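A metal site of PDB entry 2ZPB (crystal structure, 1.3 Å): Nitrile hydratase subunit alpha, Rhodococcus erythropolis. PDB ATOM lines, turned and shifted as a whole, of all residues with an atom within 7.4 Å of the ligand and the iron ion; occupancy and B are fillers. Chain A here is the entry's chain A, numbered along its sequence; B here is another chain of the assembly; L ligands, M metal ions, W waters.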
ATOM      1  N   GLN A  90     -30.706 -12.494 -19.439  1.00  0.00           N
ATOM      2  CA  GLN A  90     -29.677 -13.451 -19.856  1.00  0.00           C
ATOM      3  C   GLN A  90     -30.224 -14.476 -20.853  1.00  0.00           C
ATOM      4  O   GLN A  90     -29.757 -15.609 -20.920  1.00  0.00           O
ATOM      5  CB  GLN A  90     -29.024 -14.131 -18.648  1.00  0.00           C
ATOM      6  CG  GLN A  90     -28.244 -13.170 -17.770  1.00  0.00           C
ATOM      7  CD  GLN A  90     -27.182 -12.450 -18.564  1.00  0.00           C
ATOM      8  OE1 GLN A  90     -26.315 -13.076 -19.157  1.00  0.00           O
ATOM      9  NE2 GLN A  90     -27.268 -11.126 -18.628  1.00  0.00           N
ATOM     10  N   VAL A 108     -20.099 -23.398 -22.810  1.00  0.00           N
ATOM     11  CA  VAL A 108     -19.383 -22.958 -21.599  1.00  0.00           C
ATOM     12  C   VAL A 108     -19.367 -21.433 -21.557  1.00  0.00           C
ATOM     13  O   VAL A 108     -19.607 -20.777 -22.565  1.00  0.00           O
ATOM     14  CB  VAL A 108     -17.916 -23.527 -21.573  1.00  0.00           C
ATOM     15  CG1 VAL A 108     -17.074 -22.946 -22.689  1.00  0.00           C
ATOM     16  CG2 VAL A 108     -17.220 -23.299 -20.232  1.00  0.00           C
ATOM     17  N   CYS A 109     -19.086 -20.878 -20.380  1.00  0.00           N
ATOM     18  CA  CYS A 109     -18.652 -19.498 -20.259  1.00  0.00           C
ATOM     19  C   CYS A 109     -17.304 -19.515 -19.557  1.00  0.00           C
ATOM     20  O   CYS A 109     -17.221 -19.573 -18.321  1.00  0.00           O
ATOM     21  CB  CYS A 109     -19.640 -18.659 -19.466  1.00  0.00           C
ATOM     22  SG  CYS A 109     -19.077 -16.939 -19.286  1.00  0.00           S
ATOM     23  N   SER A 110     -16.220 -19.492 -20.324  1.00  0.00           N
ATOM     24  CA  SER A 110     -14.906 -19.674 -19.717  1.00  0.00           C
ATOM     25  C   SER A 110     -14.529 -18.477 -18.838  1.00  0.00           C
ATOM     26  O   SER A 110     -13.791 -18.644 -17.867  1.00  0.00           O
ATOM     27  CB  SER A 110     -13.819 -19.924 -20.773  1.00  0.00           C
ATOM     28  OG  SER A 110     -13.573 -18.770 -21.541  1.00  0.00           O
ATOM     29  N   LEU A 111     -15.055 -17.298 -19.163  1.00  0.00           N
ATOM     30  CA  LEU A 111     -14.666 -16.063 -18.462  1.00  0.00           C
ATOM     31  C   LEU A 111     -15.443 -15.846 -17.171  1.00  0.00           C
ATOM     32  O   LEU A 111     -15.112 -14.983 -16.362  1.00  0.00           O
ATOM     33  CB  LEU A 111     -14.816 -14.860 -19.389  1.00  0.00           C
ATOM     34  CG  LEU A 111     -13.871 -14.859 -20.587  1.00  0.00           C
ATOM     35  CD1 LEU A 111     -14.302 -13.803 -21.593  1.00  0.00           C
ATOM     36  CD2 LEU A 111     -12.428 -14.611 -20.156  1.00  0.00           C
ATOM     37  N   CSD A 112     -16.718 -16.619 -16.934  1.00  0.00           N
ATOM     38  CA  CSD A 112     -17.509 -16.415 -15.731  1.00  0.00           C
ATOM     39  CB  CSD A 112     -18.113 -15.006 -15.656  1.00  0.00           C
ATOM     40  SG  CSD A 112     -18.936 -14.426 -17.230  1.00  0.00           S
ATOM     41  C   CSD A 112     -18.554 -17.484 -15.660  1.00  0.00           C
ATOM     42  O   CSD A 112     -18.347 -18.522 -15.048  1.00  0.00           O
ATOM     43  OD1 CSD A 112     -17.840 -14.185 -18.242  1.00  0.00           O
ATOM     44  OD2 CSD A 112     -19.534 -13.158 -16.863  1.00  0.00           O
ATOM     45  N   SER A 113     -19.933 -17.310 -16.325  1.00  0.00           N
ATOM     46  CA  SER A 113     -20.931 -18.367 -16.012  1.00  0.00           C
ATOM     47  C   SER A 113     -22.084 -18.244 -16.974  1.00  0.00           C
ATOM     48  O   SER A 113     -23.099 -18.922 -16.849  1.00  0.00           O
ATOM     49  CB  SER A 113     -21.463 -18.198 -14.598  1.00  0.00           C
ATOM     50  OG  SER A 113     -22.145 -16.956 -14.472  1.00  0.00           O
ATOM     51  N   CSO A 114     -21.878 -17.230 -18.053  1.00  0.00           N
ATOM     52  CA  CSO A 114     -22.939 -16.864 -18.978  1.00  0.00           C
ATOM     53  CB  CSO A 114     -22.388 -15.970 -20.075  1.00  0.00           C
ATOM     54  SG  CSO A 114     -21.329 -14.756 -19.353  1.00  0.00           S
ATOM     55  C   CSO A 114     -23.581 -18.091 -19.581  1.00  0.00           C
ATOM     56  O   CSO A 114     -23.004 -19.101 -19.957  1.00  0.00           O
ATOM     57  OD  CSO A 114     -22.384 -13.785 -18.837  1.00  0.00           O
ATOM     58  N   THR A 115     -25.057 -18.068 -19.368  1.00  0.00           N
ATOM     59  CA  THR A 115     -26.018 -19.194 -19.524  1.00  0.00           C
ATOM     60  C   THR A 115     -27.316 -18.557 -19.956  1.00  0.00           C
ATOM     61  O   THR A 115     -27.656 -17.469 -19.502  1.00  0.00           O
ATOM     62  CB  THR A 115     -26.192 -19.912 -18.186  1.00  0.00           C
ATOM     63  OG1 THR A 115     -24.984 -20.612 -17.868  1.00  0.00           O
ATOM     64  CG2 THR A 115     -27.348 -20.892 -18.201  1.00  0.00           C
ATOM     65  N   TRP A 117     -30.316 -18.286 -19.071  1.00  0.00           N
ATOM     66  CA  TRP A 117     -31.089 -18.513 -17.835  1.00  0.00           C
ATOM     67  C   TRP A 117     -32.556 -18.915 -18.024  1.00  0.00           C
ATOM     68  O   TRP A 117     -33.009 -19.866 -17.380  1.00  0.00           O
ATOM     69  CB  TRP A 117     -31.092 -17.270 -16.945  1.00  0.00           C
ATOM     70  CG  TRP A 117     -29.799 -16.887 -16.291  1.00  0.00           C
ATOM     71  CD1 TRP A 117     -28.627 -17.593 -16.262  1.00  0.00           C
ATOM     72  CD2 TRP A 117     -29.589 -15.704 -15.526  1.00  0.00           C
ATOM     73  NE1 TRP A 117     -27.683 -16.896 -15.530  1.00  0.00           N
ATOM     74  CE2 TRP A 117     -28.251 -15.737 -15.068  1.00  0.00           C
ATOM     75  CE3 TRP A 117     -30.396 -14.616 -15.194  1.00  0.00           C
ATOM     76  CZ2 TRP A 117     -27.702 -14.707 -14.287  1.00  0.00           C
ATOM     77  CZ3 TRP A 117     -29.861 -13.603 -14.408  1.00  0.00           C
ATOM     78  CH2 TRP A 117     -28.526 -13.656 -13.963  1.00  0.00           C
ATOM     79  N   PRO A 123     -27.130 -21.398 -14.018  1.00  0.00           N
ATOM     80  CA  PRO A 123     -26.129 -22.446 -14.175  1.00  0.00           C
ATOM     81  C   PRO A 123     -25.894 -23.211 -12.872  1.00  0.00           C
ATOM     82  O   PRO A 123     -25.986 -22.633 -11.790  1.00  0.00           O
ATOM     83  CB  PRO A 123     -24.858 -21.669 -14.568  1.00  0.00           C
ATOM     84  CG  PRO A 123     -25.101 -20.275 -14.118  1.00  0.00           C
ATOM     85  CD  PRO A 123     -26.570 -20.058 -14.269  1.00  0.00           C
ATOM     86  N   TYR A 127     -20.921 -26.059 -13.627  1.00  0.00           N
ATOM     87  CA  TYR A 127     -20.714 -25.304 -14.879  1.00  0.00           C
ATOM     88  C   TYR A 127     -19.866 -24.062 -14.608  1.00  0.00           C
ATOM     89  O   TYR A 127     -19.140 -23.604 -15.479  1.00  0.00           O
ATOM     90  CB  TYR A 127     -22.072 -24.950 -15.461  1.00  0.00           C
ATOM     91  CG  TYR A 127     -22.098 -24.116 -16.714  1.00  0.00           C
ATOM     92  CD1 TYR A 127     -22.112 -22.719 -16.656  1.00  0.00           C
ATOM     93  CD2 TYR A 127     -22.167 -24.723 -17.963  1.00  0.00           C
ATOM     94  CE1 TYR A 127     -22.194 -21.954 -17.809  1.00  0.00           C
ATOM     95  CE2 TYR A 127     -22.247 -23.972 -19.117  1.00  0.00           C
ATOM     96  CZ  TYR A 127     -22.250 -22.590 -19.038  1.00  0.00           C
ATOM     97  OH  TYR A 127     -22.370 -21.838 -20.180  1.00  0.00           O
ATOM     98  N   LYS A 128     -19.999 -23.533 -13.398  1.00  0.00           N
ATOM     99  CA  LYS A 128     -19.249 -22.369 -12.944  1.00  0.00           C
ATOM    100  C   LYS A 128     -17.883 -22.728 -12.361  1.00  0.00           C
ATOM    101  O   LYS A 128     -17.104 -21.843 -12.004  1.00  0.00           O
ATOM    102  CB  LYS A 128     -20.079 -21.619 -11.899  1.00  0.00           C
ATOM    103  CG  LYS A 128     -21.412 -21.121 -12.463  1.00  0.00           C
ATOM    104  CD  LYS A 128     -22.307 -20.440 -11.454  1.00  0.00           C
ATOM    105  CE  LYS A 128     -23.063 -21.444 -10.609  1.00  0.00           C
ATOM    106  NZ  LYS A 128     -24.080 -20.815  -9.708  1.00  0.00           N
ATOM    107  N   ARG A 133     -14.525 -24.516 -16.667  1.00  0.00           N
ATOM    108  CA  ARG A 133     -14.140 -23.294 -17.371  1.00  0.00           C
ATOM    109  C   ARG A 133     -12.747 -23.398 -18.011  1.00  0.00           C
ATOM    110  O   ARG A 133     -12.528 -22.875 -19.107  1.00  0.00           O
ATOM    111  CB  ARG A 133     -14.213 -22.096 -16.422  1.00  0.00           C
ATOM    112  CG  ARG A 133     -15.655 -21.698 -16.072  1.00  0.00           C
ATOM    113  CD  ARG A 133     -15.750 -20.593 -15.028  1.00  0.00           C
ATOM    114  NE  ARG A 133     -14.885 -19.467 -15.393  1.00  0.00           N
ATOM    115  CZ  ARG A 133     -14.399 -18.553 -14.551  1.00  0.00           C
ATOM    116  NH1 ARG A 133     -14.731 -18.553 -13.259  1.00  0.00           N
ATOM    117  NH2 ARG A 133     -13.580 -17.608 -15.016  1.00  0.00           N
ATOM    118  N   THR A 162     -19.365 -18.697 -24.360  1.00  0.00           N
ATOM    119  CA  THR A 162     -20.374 -17.635 -24.266  1.00  0.00           C
ATOM    120  C   THR A 162     -19.734 -16.335 -23.797  1.00  0.00           C
ATOM    121  O   THR A 162     -19.779 -15.986 -22.614  1.00  0.00           O
ATOM    122  CB  THR A 162     -21.527 -18.082 -23.329  1.00  0.00           C
ATOM    123  OG1 THR A 162     -22.020 -19.371 -23.741  1.00  0.00           O
ATOM    124  CG2 THR A 162     -22.664 -17.084 -23.368  1.00  0.00           C
ATOM    125  N   THR A 163     -19.121 -15.611 -24.728  1.00  0.00           N
ATOM    126  CA  THR A 163     -18.267 -14.466 -24.418  1.00  0.00           C
ATOM    127  C   THR A 163     -18.933 -13.125 -24.627  1.00  0.00           C
ATOM    128  O   THR A 163     -18.362 -12.099 -24.278  1.00  0.00           O
ATOM    129  CB  THR A 163     -16.978 -14.537 -25.265  1.00  0.00           C
ATOM    130  OG1 THR A 163     -17.319 -14.811 -26.633  1.00  0.00           O
ATOM    131  CG2 THR A 163     -16.038 -15.648 -24.780  1.00  0.00           C
ATOM    132  N   ARG A 167     -26.867 -16.168 -26.267  1.00  0.00           N
ATOM    133  CA  ARG A 167     -27.118 -17.166 -25.249  1.00  0.00           C
ATOM    134  C   ARG A 167     -27.572 -18.435 -25.970  1.00  0.00           C
ATOM    135  O   ARG A 167     -28.480 -18.391 -26.802  1.00  0.00           O
ATOM    136  CB  ARG A 167     -28.164 -16.653 -24.248  1.00  0.00           C
ATOM    137  CG  ARG A 167     -27.676 -15.471 -23.427  1.00  0.00           C
ATOM    138  CD  ARG A 167     -26.668 -15.897 -22.358  1.00  0.00           C
ATOM    139  NE  ARG A 167     -26.088 -14.746 -21.655  1.00  0.00           N
ATOM    140  CZ  ARG A 167     -25.075 -14.023 -22.107  1.00  0.00           C
ATOM    141  NH1 ARG A 167     -24.474 -14.337 -23.247  1.00  0.00           N
ATOM    142  NH2 ARG A 167     -24.632 -12.990 -21.403  1.00  0.00           N
ATOM    143  N   TYR B  37     -27.409 -11.723  -7.389  1.00  0.00           N
ATOM    144  CA  TYR B  37     -28.068 -11.457  -8.680  1.00  0.00           C
ATOM    145  C   TYR B  37     -29.195 -10.437  -8.537  1.00  0.00           C
ATOM    146  O   TYR B  37     -29.343  -9.532  -9.363  1.00  0.00           O
ATOM    147  CB  TYR B  37     -28.629 -12.734  -9.324  1.00  0.00           C
ATOM    148  CG  TYR B  37     -27.641 -13.682  -9.988  1.00  0.00           C
ATOM    149  CD1 TYR B  37     -26.299 -13.346 -10.211  1.00  0.00           C
ATOM    150  CD2 TYR B  37     -28.091 -14.924 -10.444  1.00  0.00           C
ATOM    151  CE1 TYR B  37     -25.425 -14.239 -10.852  1.00  0.00           C
ATOM    152  CE2 TYR B  37     -27.235 -15.805 -11.077  1.00  0.00           C
ATOM    153  CZ  TYR B  37     -25.915 -15.461 -11.274  1.00  0.00           C
ATOM    154  OH  TYR B  37     -25.098 -16.375 -11.910  1.00  0.00           O
ATOM    155  N   MET B  40     -27.672  -7.076  -8.011  1.00  0.00           N
ATOM    156  CA  MET B  40     -27.127  -6.642  -9.292  1.00  0.00           C
ATOM    157  C   MET B  40     -28.216  -5.981 -10.128  1.00  0.00           C
ATOM    158  O   MET B  40     -28.023  -4.890 -10.658  1.00  0.00           O
ATOM    159  CB  MET B  40     -26.502  -7.808 -10.063  1.00  0.00           C
ATOM    160  CG  MET B  40     -26.068  -7.415 -11.470  1.00  0.00           C
ATOM    161  SD  MET B  40     -25.269  -8.737 -12.379  1.00  0.00           S
ATOM    162  CE  MET B  40     -26.656  -9.844 -12.654  1.00  0.00           C
ATOM    163  N   VAL B  52     -24.261  -4.398 -16.399  1.00  0.00           N
ATOM    164  CA  VAL B  52     -23.841  -5.781 -16.161  1.00  0.00           C
ATOM    165  C   VAL B  52     -22.338  -5.929 -16.491  1.00  0.00           C
ATOM    166  O   VAL B  52     -21.610  -6.634 -15.778  1.00  0.00           O
ATOM    167  CB  VAL B  52     -24.719  -6.800 -16.947  1.00  0.00           C
ATOM    168  CG1 VAL B  52     -24.189  -8.218 -16.781  1.00  0.00           C
ATOM    169  CG2 VAL B  52     -26.184  -6.713 -16.482  1.00  0.00           C
ATOM    170  N   ARG B  56     -19.170  -7.702 -14.339  1.00  0.00           N
ATOM    171  CA  ARG B  56     -18.148  -8.657 -14.788  1.00  0.00           C
ATOM    172  C   ARG B  56     -16.755  -8.121 -14.471  1.00  0.00           C
ATOM    173  O   ARG B  56     -15.920  -8.845 -13.912  1.00  0.00           O
ATOM    174  CB  ARG B  56     -18.260  -8.938 -16.279  1.00  0.00           C
ATOM    175  CG  ARG B  56     -19.553  -9.617 -16.676  1.00  0.00           C
ATOM    176  CD  ARG B  56     -19.433 -10.204 -18.074  1.00  0.00           C
ATOM    177  NE  ARG B  56     -20.691 -10.879 -18.410  1.00  0.00           N
ATOM    178  CZ  ARG B  56     -21.730 -10.279 -18.983  1.00  0.00           C
ATOM    179  NH1 ARG B  56     -21.669  -9.005 -19.321  1.00  0.00           N
ATOM    180  NH2 ARG B  56     -22.852 -10.964 -19.216  1.00  0.00           N
ATOM    181  N   TYR B  72     -18.401 -18.950  -6.287  1.00  0.00           N
ATOM    182  CA  TYR B  72     -19.028 -18.132  -7.301  1.00  0.00           C
ATOM    183  C   TYR B  72     -19.971 -17.037  -6.751  1.00  0.00           C
ATOM    184  O   TYR B  72     -19.779 -15.847  -7.028  1.00  0.00           O
ATOM    185  CB  TYR B  72     -19.765 -19.039  -8.286  1.00  0.00           C
ATOM    186  CG  TYR B  72     -20.527 -18.245  -9.305  1.00  0.00           C
ATOM    187  CD1 TYR B  72     -19.921 -17.850 -10.494  1.00  0.00           C
ATOM    188  CD2 TYR B  72     -21.847 -17.874  -9.085  1.00  0.00           C
ATOM    189  CE1 TYR B  72     -20.605 -17.106 -11.429  1.00  0.00           C
ATOM    190  CE2 TYR B  72     -22.548 -17.118 -10.013  1.00  0.00           C
ATOM    191  CZ  TYR B  72     -21.921 -16.744 -11.189  1.00  0.00           C
ATOM    192  OH  TYR B  72     -22.605 -16.000 -12.125  1.00  0.00           O
ATOM    193  N   TYR B  76     -19.828 -12.441  -6.525  1.00  0.00           N
ATOM    194  CA  TYR B  76     -20.795 -11.410  -6.904  1.00  0.00           C
ATOM    195  C   TYR B  76     -21.259 -10.534  -5.763  1.00  0.00           C
ATOM    196  O   TYR B  76     -21.509  -9.349  -5.969  1.00  0.00           O
ATOM    197  CB  TYR B  76     -21.936 -11.997  -7.739  1.00  0.00           C
ATOM    198  CG  TYR B  76     -21.338 -12.495  -9.031  1.00  0.00           C
ATOM    199  CD1 TYR B  76     -21.280 -11.685 -10.175  1.00  0.00           C
ATOM    200  CD2 TYR B  76     -20.680 -13.722  -9.067  1.00  0.00           C
ATOM    201  CE1 TYR B  76     -20.643 -12.134 -11.346  1.00  0.00           C
ATOM    202  CE2 TYR B  76     -20.046 -14.170 -10.197  1.00  0.00           C
ATOM    203  CZ  TYR B  76     -20.030 -13.394 -11.335  1.00  0.00           C
ATOM    204  OH  TYR B  76     -19.384 -13.916 -12.432  1.00  0.00           O
ATOM    205  N   ARG B 141     -13.933  -8.682 -23.624  1.00  0.00           N
ATOM    206  CA  ARG B 141     -14.633  -9.963 -23.772  1.00  0.00           C
ATOM    207  C   ARG B 141     -13.975 -10.831 -24.845  1.00  0.00           C
ATOM    208  O   ARG B 141     -14.635 -11.435 -25.693  1.00  0.00           O
ATOM    209  CB  ARG B 141     -16.114  -9.747 -24.050  1.00  0.00           C
ATOM    210  CG  ARG B 141     -16.866  -9.123 -22.891  1.00  0.00           C
ATOM    211  CD  ARG B 141     -16.722  -9.938 -21.617  1.00  0.00           C
ATOM    212  NE  ARG B 141     -17.419 -11.225 -21.713  1.00  0.00           N
ATOM    213  CZ  ARG B 141     -17.464 -12.121 -20.735  1.00  0.00           C
ATOM    214  NH1 ARG B 141     -16.768 -11.924 -19.616  1.00  0.00           N
ATOM    215  NH2 ARG B 141     -18.180 -13.217 -20.890  1.00  0.00           N
HETATM  216  N1  LIG L   1     -21.676 -14.934 -16.274  1.00  0.00           N
HETATM  217  O1  LIG L   1     -23.073 -14.627 -16.508  1.00  0.00           O
HETATM  218 FE    FE M   1     -20.424 -15.933 -17.682  1.00  0.00          FE
HETATM  219  O   HOH W   1     -24.804 -17.066 -15.764  1.00  0.00           O
HETATM  220  O   HOH W   2     -25.863 -15.584 -17.987  1.00  0.00           O
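The side-chain hydroxyl (OG) of Ser 113 sits at hydrogen-bond distance from an oxygen (O1) of the ligand, at 3.2 Å.
The guanidinium group (NH2) of Arg 141 of chain B is in salt-bridge range of OD1 of CSD 112 (2.8 Å). The backbone NH (N) of Cys 109 is in hydrogen-bond range of the side-chain hydroxyl (OH) of Tyr 127 (3.4 Å). The side-chain sulfur of Cys 109 sits close to the backbone carbonyl oxygen of Thr 162, 3.5 Å away. O of CSO 114 sits at hydrogen-bond distance from the side-chain hydroxyl of Tyr 127, 2.8 Å away. OG of Ser 113 is in hydrogen-bond range of OH of Tyr 72 of chain B (2.6 Å). The backbone carbonyl oxygen of Ser 113 lies within hydrogen-bond range of the side-chain hydroxyl of Thr 115. OD of CSO 114 is in hydrogen-bond range of NH2 of Arg 56 of chain B (2.9 Å). OD2 of CSD 112 is in salt-bridge range of the guanidinium group (NE) of Arg 56 of chain B.
Of the 24 residues printed, 3 come within 4 Å of the ligand.
Within 4 Å of the iron ion: Cys 109, CSD 112, Ser 113 and CSO 114. The nearest printed residue that does not touch the iron ion is Arg 141 of chain B (4.8 Å).
The iron ion is bound by N of CSO 114 (2.0 Å), the backbone nitrogen of Ser 113 (2.0 Å), a nitrogen (N1) of the ligand (2.1 Å), SG of CSD 112 (2.2 Å), SG of CSO 114 (2.2 Å) and the side-chain sulfur of Cys 109 (2.3 Å). The iron ion has six donor atoms within binding distance.
Water W1 lies within hydrogen-bond range of O of Ser 113 (2.7 Å), NE1 of Trp 117 (2.9 Å) and O1 of the ligand (3.1 Å). Water W2 lies within hydrogen-bond range of OE1 of Gln 90 (2.8 Å), N of Thr 115 (3.0 Å), O1 of the ligand (3.3 Å) and NE1 of Trp 117 (3.3 Å).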
